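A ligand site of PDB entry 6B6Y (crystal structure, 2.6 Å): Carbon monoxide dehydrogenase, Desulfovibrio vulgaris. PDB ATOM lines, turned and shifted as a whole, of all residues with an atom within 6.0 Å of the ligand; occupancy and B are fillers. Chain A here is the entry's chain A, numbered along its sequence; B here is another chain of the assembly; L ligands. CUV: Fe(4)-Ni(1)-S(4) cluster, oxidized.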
ATOM      1  N   HIS A 105      -8.434  24.205  26.819  1.00  0.00           N
ATOM      2  CA  HIS A 105      -8.849  22.988  26.141  1.00  0.00           C
ATOM      3  C   HIS A 105      -8.572  21.761  27.002  1.00  0.00           C
ATOM      4  O   HIS A 105      -9.403  20.849  27.071  1.00  0.00           O
ATOM      5  CB  HIS A 105      -8.130  22.881  24.799  1.00  0.00           C
ATOM      6  CG  HIS A 105      -8.498  23.954  23.835  1.00  0.00           C
ATOM      7  ND1 HIS A 105      -7.579  24.560  23.006  1.00  0.00           N
ATOM      8  CD2 HIS A 105      -9.682  24.562  23.583  1.00  0.00           C
ATOM      9  CE1 HIS A 105      -8.183  25.477  22.271  1.00  0.00           C
ATOM     10  NE2 HIS A 105      -9.458  25.495  22.604  1.00  0.00           N
ATOM     11  N   GLY A 273     -20.881  28.809  26.360  1.00  0.00           N
ATOM     12  CA  GLY A 273     -19.678  28.188  26.867  1.00  0.00           C
ATOM     13  C   GLY A 273     -19.145  27.091  25.968  1.00  0.00           C
ATOM     14  O   GLY A 273     -18.987  27.289  24.764  1.00  0.00           O
ATOM     15  N   HIS A 274     -18.876  25.903  26.544  1.00  0.00           N
ATOM     16  CA  HIS A 274     -18.170  24.844  25.833  1.00  0.00           C
ATOM     17  C   HIS A 274     -18.653  23.432  26.114  1.00  0.00           C
ATOM     18  O   HIS A 274     -18.583  22.595  25.210  1.00  0.00           O
ATOM     19  CB  HIS A 274     -16.661  24.902  26.135  1.00  0.00           C
ATOM     20  CG  HIS A 274     -15.949  26.025  25.432  1.00  0.00           C
ATOM     21  ND1 HIS A 274     -16.107  27.344  25.804  1.00  0.00           N
ATOM     22  CD2 HIS A 274     -15.075  26.012  24.406  1.00  0.00           C
ATOM     23  CE1 HIS A 274     -15.352  28.103  25.017  1.00  0.00           C
ATOM     24  NE2 HIS A 274     -14.727  27.319  24.162  1.00  0.00           N
ATOM     25  N   CYS A 309     -21.593  30.402  21.384  1.00  0.00           N
ATOM     26  CA  CYS A 309     -20.160  30.074  21.537  1.00  0.00           C
ATOM     27  C   CYS A 309     -19.915  28.652  21.005  1.00  0.00           C
ATOM     28  O   CYS A 309     -20.472  28.269  19.974  1.00  0.00           O
ATOM     29  CB  CYS A 309     -19.703  30.339  22.962  1.00  0.00           C
ATOM     30  SG  CYS A 309     -17.916  30.305  23.225  1.00  0.00           S
ATOM     31  N   CYS A 310     -19.092  27.857  21.701  1.00  0.00           N
ATOM     32  CA  CYS A 310     -18.683  26.541  21.239  1.00  0.00           C
ATOM     33  C   CYS A 310     -19.685  25.449  21.606  1.00  0.00           C
ATOM     34  O   CYS A 310     -19.898  24.515  20.834  1.00  0.00           O
ATOM     35  CB  CYS A 310     -17.289  26.212  21.764  1.00  0.00           C
ATOM     36  SG  CYS A 310     -15.938  26.967  20.811  1.00  0.00           S
ATOM     37  N   THR A 311     -20.289  25.538  22.799  1.00  0.00           N
ATOM     38  CA  THR A 311     -21.351  24.597  23.150  1.00  0.00           C
ATOM     39  C   THR A 311     -22.531  24.714  22.180  1.00  0.00           C
ATOM     40  O   THR A 311     -23.243  23.734  21.946  1.00  0.00           O
ATOM     41  CB  THR A 311     -21.780  24.816  24.607  1.00  0.00           C
ATOM     42  OG1 THR A 311     -22.758  23.830  24.972  1.00  0.00           O
ATOM     43  CG2 THR A 311     -22.363  26.200  24.805  1.00  0.00           C
ATOM     44  N   ASN A 313     -22.081  25.741  18.866  1.00  0.00           N
ATOM     45  CA  ASN A 313     -21.486  25.094  17.707  1.00  0.00           C
ATOM     46  C   ASN A 313     -21.650  23.579  17.774  1.00  0.00           C
ATOM     47  O   ASN A 313     -22.028  22.937  16.782  1.00  0.00           O
ATOM     48  CB  ASN A 313     -19.990  25.438  17.621  1.00  0.00           C
ATOM     49  CG  ASN A 313     -19.701  26.626  16.736  1.00  0.00           C
ATOM     50  OD1 ASN A 313     -19.648  26.506  15.505  1.00  0.00           O
ATOM     51  ND2 ASN A 313     -19.481  27.780  17.349  1.00  0.00           N
ATOM     52  N   ASN A 326     -22.434  34.601  17.671  1.00  0.00           N
ATOM     53  CA  ASN A 326     -21.063  34.326  18.075  1.00  0.00           C
ATOM     54  C   ASN A 326     -20.646  35.162  19.274  1.00  0.00           C
ATOM     55  O   ASN A 326     -21.489  35.574  20.078  1.00  0.00           O
ATOM     56  CB  ASN A 326     -20.112  34.493  16.886  1.00  0.00           C
ATOM     57  CG  ASN A 326     -20.317  35.791  16.140  1.00  0.00           C
ATOM     58  OD1 ASN A 326     -20.757  36.792  16.719  1.00  0.00           O
ATOM     59  ND2 ASN A 326     -20.026  35.778  14.856  1.00  0.00           N
ATOM     60  N   HIS A 327     -19.340  35.426  19.395  1.00  0.00           N
ATOM     61  CA  HIS A 327     -18.769  36.037  20.600  1.00  0.00           C
ATOM     62  C   HIS A 327     -19.422  37.372  20.927  1.00  0.00           C
ATOM     63  O   HIS A 327     -19.940  37.570  22.033  1.00  0.00           O
ATOM     64  CB  HIS A 327     -17.259  36.188  20.432  1.00  0.00           C
ATOM     65  CG  HIS A 327     -16.580  36.895  21.570  1.00  0.00           C
ATOM     66  ND1 HIS A 327     -16.789  36.546  22.889  1.00  0.00           N
ATOM     67  CD2 HIS A 327     -15.713  37.934  21.587  1.00  0.00           C
ATOM     68  CE1 HIS A 327     -16.069  37.333  23.671  1.00  0.00           C
ATOM     69  NE2 HIS A 327     -15.411  38.182  22.903  1.00  0.00           N
ATOM     70  N   GLN A 347     -15.210  29.239  29.981  1.00  0.00           N
ATOM     71  CA  GLN A 347     -14.476  29.678  28.792  1.00  0.00           C
ATOM     72  C   GLN A 347     -15.267  30.624  27.889  1.00  0.00           C
ATOM     73  O   GLN A 347     -16.338  30.258  27.373  1.00  0.00           O
ATOM     74  CB  GLN A 347     -13.900  28.497  28.003  1.00  0.00           C
ATOM     75  CG  GLN A 347     -12.837  27.710  28.743  1.00  0.00           C
ATOM     76  CD  GLN A 347     -11.585  28.521  29.000  1.00  0.00           C
ATOM     77  OE1 GLN A 347     -10.861  28.862  28.063  1.00  0.00           O
ATOM     78  NE2 GLN A 347     -11.323  28.837  30.261  1.00  0.00           N
ATOM     79  N   CYS A 348     -14.749  31.845  27.715  1.00  0.00           N
ATOM     80  CA  CYS A 348     -15.257  32.838  26.761  1.00  0.00           C
ATOM     81  C   CYS A 348     -16.625  33.396  27.132  1.00  0.00           C
ATOM     82  O   CYS A 348     -17.323  33.937  26.274  1.00  0.00           O
ATOM     83  CB  CYS A 348     -15.237  32.332  25.323  1.00  0.00           C
ATOM     84  SG  CYS A 348     -13.624  31.772  24.797  1.00  0.00           S
ATOM     85  N   VAL A 454     -10.439  29.903  11.818  1.00  0.00           N
ATOM     86  CA  VAL A 454     -10.667  29.605  13.232  1.00  0.00           C
ATOM     87  C   VAL A 454     -11.100  30.836  14.004  1.00  0.00           C
ATOM     88  O   VAL A 454     -11.206  30.780  15.234  1.00  0.00           O
ATOM     89  CB  VAL A 454      -9.438  28.938  13.871  1.00  0.00           C
ATOM     90  CG1 VAL A 454      -8.975  27.770  13.018  1.00  0.00           C
ATOM     91  CG2 VAL A 454      -8.313  29.935  14.008  1.00  0.00           C
ATOM     92  N   GLY A 455     -11.357  31.951  13.333  1.00  0.00           N
ATOM     93  CA  GLY A 455     -11.409  33.249  13.992  1.00  0.00           C
ATOM     94  C   GLY A 455     -12.472  33.347  15.079  1.00  0.00           C
ATOM     95  O   GLY A 455     -13.421  32.562  15.166  1.00  0.00           O
ATOM     96  N   CYS A 456     -12.274  34.347  15.935  1.00  0.00           N
ATOM     97  CA  CYS A 456     -13.262  34.772  16.909  1.00  0.00           C
ATOM     98  C   CYS A 456     -13.909  36.064  16.440  1.00  0.00           C
ATOM     99  O   CYS A 456     -14.107  36.270  15.243  1.00  0.00           O
ATOM    100  CB  CYS A 456     -12.596  35.065  18.258  1.00  0.00           C
ATOM    101  SG  CYS A 456     -11.299  33.954  18.807  1.00  0.00           S
ATOM    102  N   ASN A 457     -14.215  36.936  17.393  1.00  0.00           N
ATOM    103  CA  ASN A 457     -14.524  38.325  17.134  1.00  0.00           C
ATOM    104  C   ASN A 457     -13.650  39.168  18.052  1.00  0.00           C
ATOM    105  O   ASN A 457     -13.222  38.713  19.113  1.00  0.00           O
ATOM    106  CB  ASN A 457     -15.990  38.644  17.419  1.00  0.00           C
ATOM    107  CG  ASN A 457     -16.909  38.130  16.343  1.00  0.00           C
ATOM    108  OD1 ASN A 457     -17.804  37.345  16.611  1.00  0.00           O
ATOM    109  ND2 ASN A 457     -16.694  38.594  15.111  1.00  0.00           N
ATOM    110  N   THR A 484     -14.771  26.822  11.878  1.00  0.00           N
ATOM    111  CA  THR A 484     -15.082  26.446  13.248  1.00  0.00           C
ATOM    112  C   THR A 484     -15.290  27.714  14.067  1.00  0.00           C
ATOM    113  O   THR A 484     -15.000  28.819  13.608  1.00  0.00           O
ATOM    114  CB  THR A 484     -13.937  25.656  13.911  1.00  0.00           C
ATOM    115  OG1 THR A 484     -12.832  26.534  14.140  1.00  0.00           O
ATOM    116  CG2 THR A 484     -13.498  24.468  13.062  1.00  0.00           C
ATOM    117  N   GLY A 485     -15.818  27.538  15.272  1.00  0.00           N
ATOM    118  CA  GLY A 485     -15.868  28.647  16.208  1.00  0.00           C
ATOM    119  C   GLY A 485     -16.829  29.741  15.773  1.00  0.00           C
ATOM    120  O   GLY A 485     -17.975  29.484  15.401  1.00  0.00           O
ATOM    121  N   CYS A 486     -16.344  30.992  15.831  1.00  0.00           N
ATOM    122  CA  CYS A 486     -17.203  32.140  15.567  1.00  0.00           C
ATOM    123  C   CYS A 486     -17.516  32.304  14.086  1.00  0.00           C
ATOM    124  O   CYS A 486     -18.611  32.741  13.713  1.00  0.00           O
ATOM    125  CB  CYS A 486     -16.550  33.413  16.112  1.00  0.00           C
ATOM    126  SG  CYS A 486     -16.810  33.702  17.870  1.00  0.00           S
ATOM    127  N   VAL A 487     -16.542  31.980  13.214  1.00  0.00           N
ATOM    128  CA  VAL A 487     -16.737  32.115  11.780  1.00  0.00           C
ATOM    129  C   VAL A 487     -17.946  31.332  11.301  1.00  0.00           C
ATOM    130  O   VAL A 487     -18.483  31.627  10.227  1.00  0.00           O
ATOM    131  CB  VAL A 487     -15.450  31.676  11.036  1.00  0.00           C
ATOM    132  CG1 VAL A 487     -15.507  32.072   9.560  1.00  0.00           C
ATOM    133  CG2 VAL A 487     -14.234  32.285  11.718  1.00  0.00           C
ATOM    134  N   SER A 526     -16.633  23.476  16.832  1.00  0.00           N
ATOM    135  CA  SER A 526     -16.236  24.498  17.781  1.00  0.00           C
ATOM    136  C   SER A 526     -14.717  24.675  17.752  1.00  0.00           C
ATOM    137  O   SER A 526     -14.009  24.137  16.902  1.00  0.00           O
ATOM    138  CB  SER A 526     -16.703  24.035  19.145  1.00  0.00           C
ATOM    139  OG  SER A 526     -16.099  22.796  19.465  1.00  0.00           O
ATOM    140  N   CYS A 527     -14.196  25.458  18.707  1.00  0.00           N
ATOM    141  CA  CYS A 527     -12.752  25.640  18.779  1.00  0.00           C
ATOM    142  C   CYS A 527     -12.043  24.340  19.100  1.00  0.00           C
ATOM    143  O   CYS A 527     -10.935  24.087  18.602  1.00  0.00           O
ATOM    144  CB  CYS A 527     -12.394  26.706  19.816  1.00  0.00           C
ATOM    145  SG  CYS A 527     -12.304  28.354  19.131  1.00  0.00           S
ATOM    146  N   VAL A 528     -12.645  23.502  19.941  1.00  0.00           N
ATOM    147  CA  VAL A 528     -12.039  22.211  20.234  1.00  0.00           C
ATOM    148  C   VAL A 528     -11.944  21.383  18.975  1.00  0.00           C
ATOM    149  O   VAL A 528     -10.936  20.708  18.720  1.00  0.00           O
ATOM    150  CB  VAL A 528     -12.844  21.490  21.342  1.00  0.00           C
ATOM    151  CG1 VAL A 528     -12.301  20.095  21.559  1.00  0.00           C
ATOM    152  CG2 VAL A 528     -12.804  22.292  22.621  1.00  0.00           C
ATOM    153  N   TYR A 561      -8.998  36.704  19.449  1.00  0.00           N
ATOM    154  CA  TYR A 561      -8.755  37.464  20.668  1.00  0.00           C
ATOM    155  C   TYR A 561      -8.193  36.650  21.827  1.00  0.00           C
ATOM    156  O   TYR A 561      -7.502  37.218  22.685  1.00  0.00           O
ATOM    157  CB  TYR A 561     -10.028  38.198  21.152  1.00  0.00           C
ATOM    158  CG  TYR A 561     -10.878  37.342  22.075  1.00  0.00           C
ATOM    159  CD1 TYR A 561     -11.778  36.422  21.552  1.00  0.00           C
ATOM    160  CD2 TYR A 561     -10.767  37.447  23.453  1.00  0.00           C
ATOM    161  CE1 TYR A 561     -12.535  35.625  22.385  1.00  0.00           C
ATOM    162  CE2 TYR A 561     -11.527  36.651  24.296  1.00  0.00           C
ATOM    163  CZ  TYR A 561     -12.419  35.743  23.753  1.00  0.00           C
ATOM    164  OH  TYR A 561     -13.182  34.944  24.563  1.00  0.00           O
ATOM    165  N   SER A 562      -8.459  35.347  21.909  1.00  0.00           N
ATOM    166  CA  SER A 562      -8.306  34.577  23.137  1.00  0.00           C
ATOM    167  C   SER A 562      -7.024  33.750  23.137  1.00  0.00           C
ATOM    168  O   SER A 562      -6.416  33.476  22.094  1.00  0.00           O
ATOM    169  CB  SER A 562      -9.500  33.625  23.312  1.00  0.00           C
ATOM    170  OG  SER A 562      -9.539  32.678  22.251  1.00  0.00           O
ATOM    171  N   LYS A 564      -6.960  30.645  23.721  1.00  0.00           N
ATOM    172  CA  LYS A 564      -7.262  29.414  23.000  1.00  0.00           C
ATOM    173  C   LYS A 564      -7.048  29.562  21.501  1.00  0.00           C
ATOM    174  O   LYS A 564      -6.632  28.610  20.822  1.00  0.00           O
ATOM    175  CB  LYS A 564      -8.683  28.937  23.310  1.00  0.00           C
ATOM    176  CG  LYS A 564      -8.914  28.682  24.793  1.00  0.00           C
ATOM    177  CD  LYS A 564     -10.159  27.835  25.089  1.00  0.00           C
ATOM    178  CE  LYS A 564     -11.463  28.617  24.903  1.00  0.00           C
ATOM    179  NZ  LYS A 564     -11.962  28.589  23.492  1.00  0.00           N
ATOM    180  N   ALA A 565      -7.298  30.752  20.953  1.00  0.00           N
ATOM    181  CA  ALA A 565      -7.048  30.985  19.543  1.00  0.00           C
ATOM    182  C   ALA A 565      -5.544  30.961  19.241  1.00  0.00           C
ATOM    183  O   ALA A 565      -5.127  30.412  18.221  1.00  0.00           O
ATOM    184  CB  ALA A 565      -7.665  32.307  19.114  1.00  0.00           C
ATOM    185  N   ILE A 568      -4.369  27.426  19.336  1.00  0.00           N
ATOM    186  CA  ILE A 568      -4.758  26.775  18.084  1.00  0.00           C
ATOM    187  C   ILE A 568      -3.824  27.213  16.968  1.00  0.00           C
ATOM    188  O   ILE A 568      -3.318  26.383  16.191  1.00  0.00           O
ATOM    189  CB  ILE A 568      -6.234  27.033  17.761  1.00  0.00           C
ATOM    190  CG1 ILE A 568      -7.137  26.223  18.703  1.00  0.00           C
ATOM    191  CG2 ILE A 568      -6.551  26.680  16.301  1.00  0.00           C
ATOM    192  CD1 ILE A 568      -8.552  26.761  18.833  1.00  0.00           C
ATOM    193  N   HIS B 210      -8.183  31.955  32.297  1.00  0.00           N
ATOM    194  CA  HIS B 210      -8.530  32.337  30.931  1.00  0.00           C
ATOM    195  C   HIS B 210      -9.787  33.192  30.948  1.00  0.00           C
ATOM    196  O   HIS B 210     -10.639  33.072  31.846  1.00  0.00           O
ATOM    197  CB  HIS B 210      -8.771  31.077  30.086  1.00  0.00           C
ATOM    198  CG  HIS B 210      -8.993  31.346  28.628  1.00  0.00           C
ATOM    199  ND1 HIS B 210     -10.193  31.790  28.130  1.00  0.00           N
ATOM    200  CD2 HIS B 210      -8.174  31.196  27.564  1.00  0.00           C
ATOM    201  CE1 HIS B 210     -10.109  31.932  26.819  1.00  0.00           C
ATOM    202  NE2 HIS B 210      -8.890  31.579  26.447  1.00  0.00           N
HETATM  203 NI   CUV L   1     -14.047  28.112  22.145  1.00  0.00          NI
HETATM  204  S1  CUV L   1     -13.822  31.053  17.885  1.00  0.00           S
HETATM  205  S2  CUV L   1     -14.580  33.119  21.094  1.00  0.00           S
HETATM  206  S3  CUV L   1     -17.110  30.045  19.267  1.00  0.00           S
HETATM  207  S4  CUV L   1     -11.526  30.809  21.429  1.00  0.00           S
HETATM  208 FE1  CUV L   1     -13.776  31.253  22.354  1.00  0.00          FE
HETATM  209 FE2  CUV L   1     -16.218  29.675  21.484  1.00  0.00          FE
HETATM  210 FE3  CUV L   1     -12.702  32.138  19.798  1.00  0.00          FE
HETATM  211 FE4  CUV L   1     -15.631  31.942  19.215  1.00  0.00          FE
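NE2 of His 274 is bound to NI of the ligand. FE3 of the ligand is bound by SG of Cys 456 (2.5 Å). An iron atom (FE1) of the ligand is bound by the side-chain sulfur (SG) of Cys 348. The backbone NH (N) of Cys 486 sits close to a sulfur (S1) of the ligand (3.3 Å). FE4 of the ligand is bound by SG of Cys 486. The side-chain sulfur of Cys 309 is bound to an iron atom (FE2) of the ligand, at 2.5 Å. A nickel atom (NI) of the ligand is bound by the side-chain amino group (NZ) of Lys 564 (2.5 Å). A nickel atom (NI) of the ligand is bound by the side-chain sulfur of Cys 310 (2.6 Å). OG of Ser 562 sits close to S4 of the ligand, at 2.8 Å. The side-chain sulfur of Cys 527 lies close to a sulfur (S1) of the ligand, at 3.3 Å. The side-chain amide nitrogen (ND2) of Asn 313 sits close to a sulfur (S3) of the ligand, at 3.8 Å.
The backbone carbonyl oxygen (O) of Val 454 lies close to a sulfur (S1) of the ligand, 3.7 Å away. The backbone carbonyl oxygen (O) of Gly 455 sits close to a sulfur (S1) of the ligand (3.1 Å). C of Gly 485 touches S3 of the ligand (3.5 Å). Tyr 561 touches the ligand. Hydrophobic or aromatic side chains within 4 Å of the ligand: His 274 and Tyr 561. Within 4 Å of the ligand: His 274, Cys 309, Cys 310, Asn 313, Cys 348, Val 454, Gly 455, Cys 456, Gly 485, Cys 486, Cys 527, Tyr 561, Ser 562 and Lys 564. The nearest printed residue that does not touch the ligand is His 327 (4.1 Å).
The side-chain sulfur (SG) of Cys 456 sits close to the backbone NH (N) of Tyr 561 (3.6 Å). N of Cys 486 sits close to O of Gly 455 (3.4 Å). The backbone carbonyl oxygen (O) of Cys 309 lies within hydrogen-bond range of the side-chain amide nitrogen (ND2) of Asn 313, 2.8 Å away. O of Gly 273 sits close to SG of Cys 309. SG of Cys 310 lies close to N of Cys 527, 3.1 Å away. The backbone NH (N) of Cys 310 sits at hydrogen-bond distance from the backbone carbonyl oxygen (O) of Gly 273 (3.1 Å). OG of Ser 562 is in hydrogen-bond range of N of Ala 565. The backbone carbonyl oxygen (O) of Gly 485 is in hydrogen-bond range of the side-chain amide nitrogen (ND2) of Asn 313 (3.0 Å).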
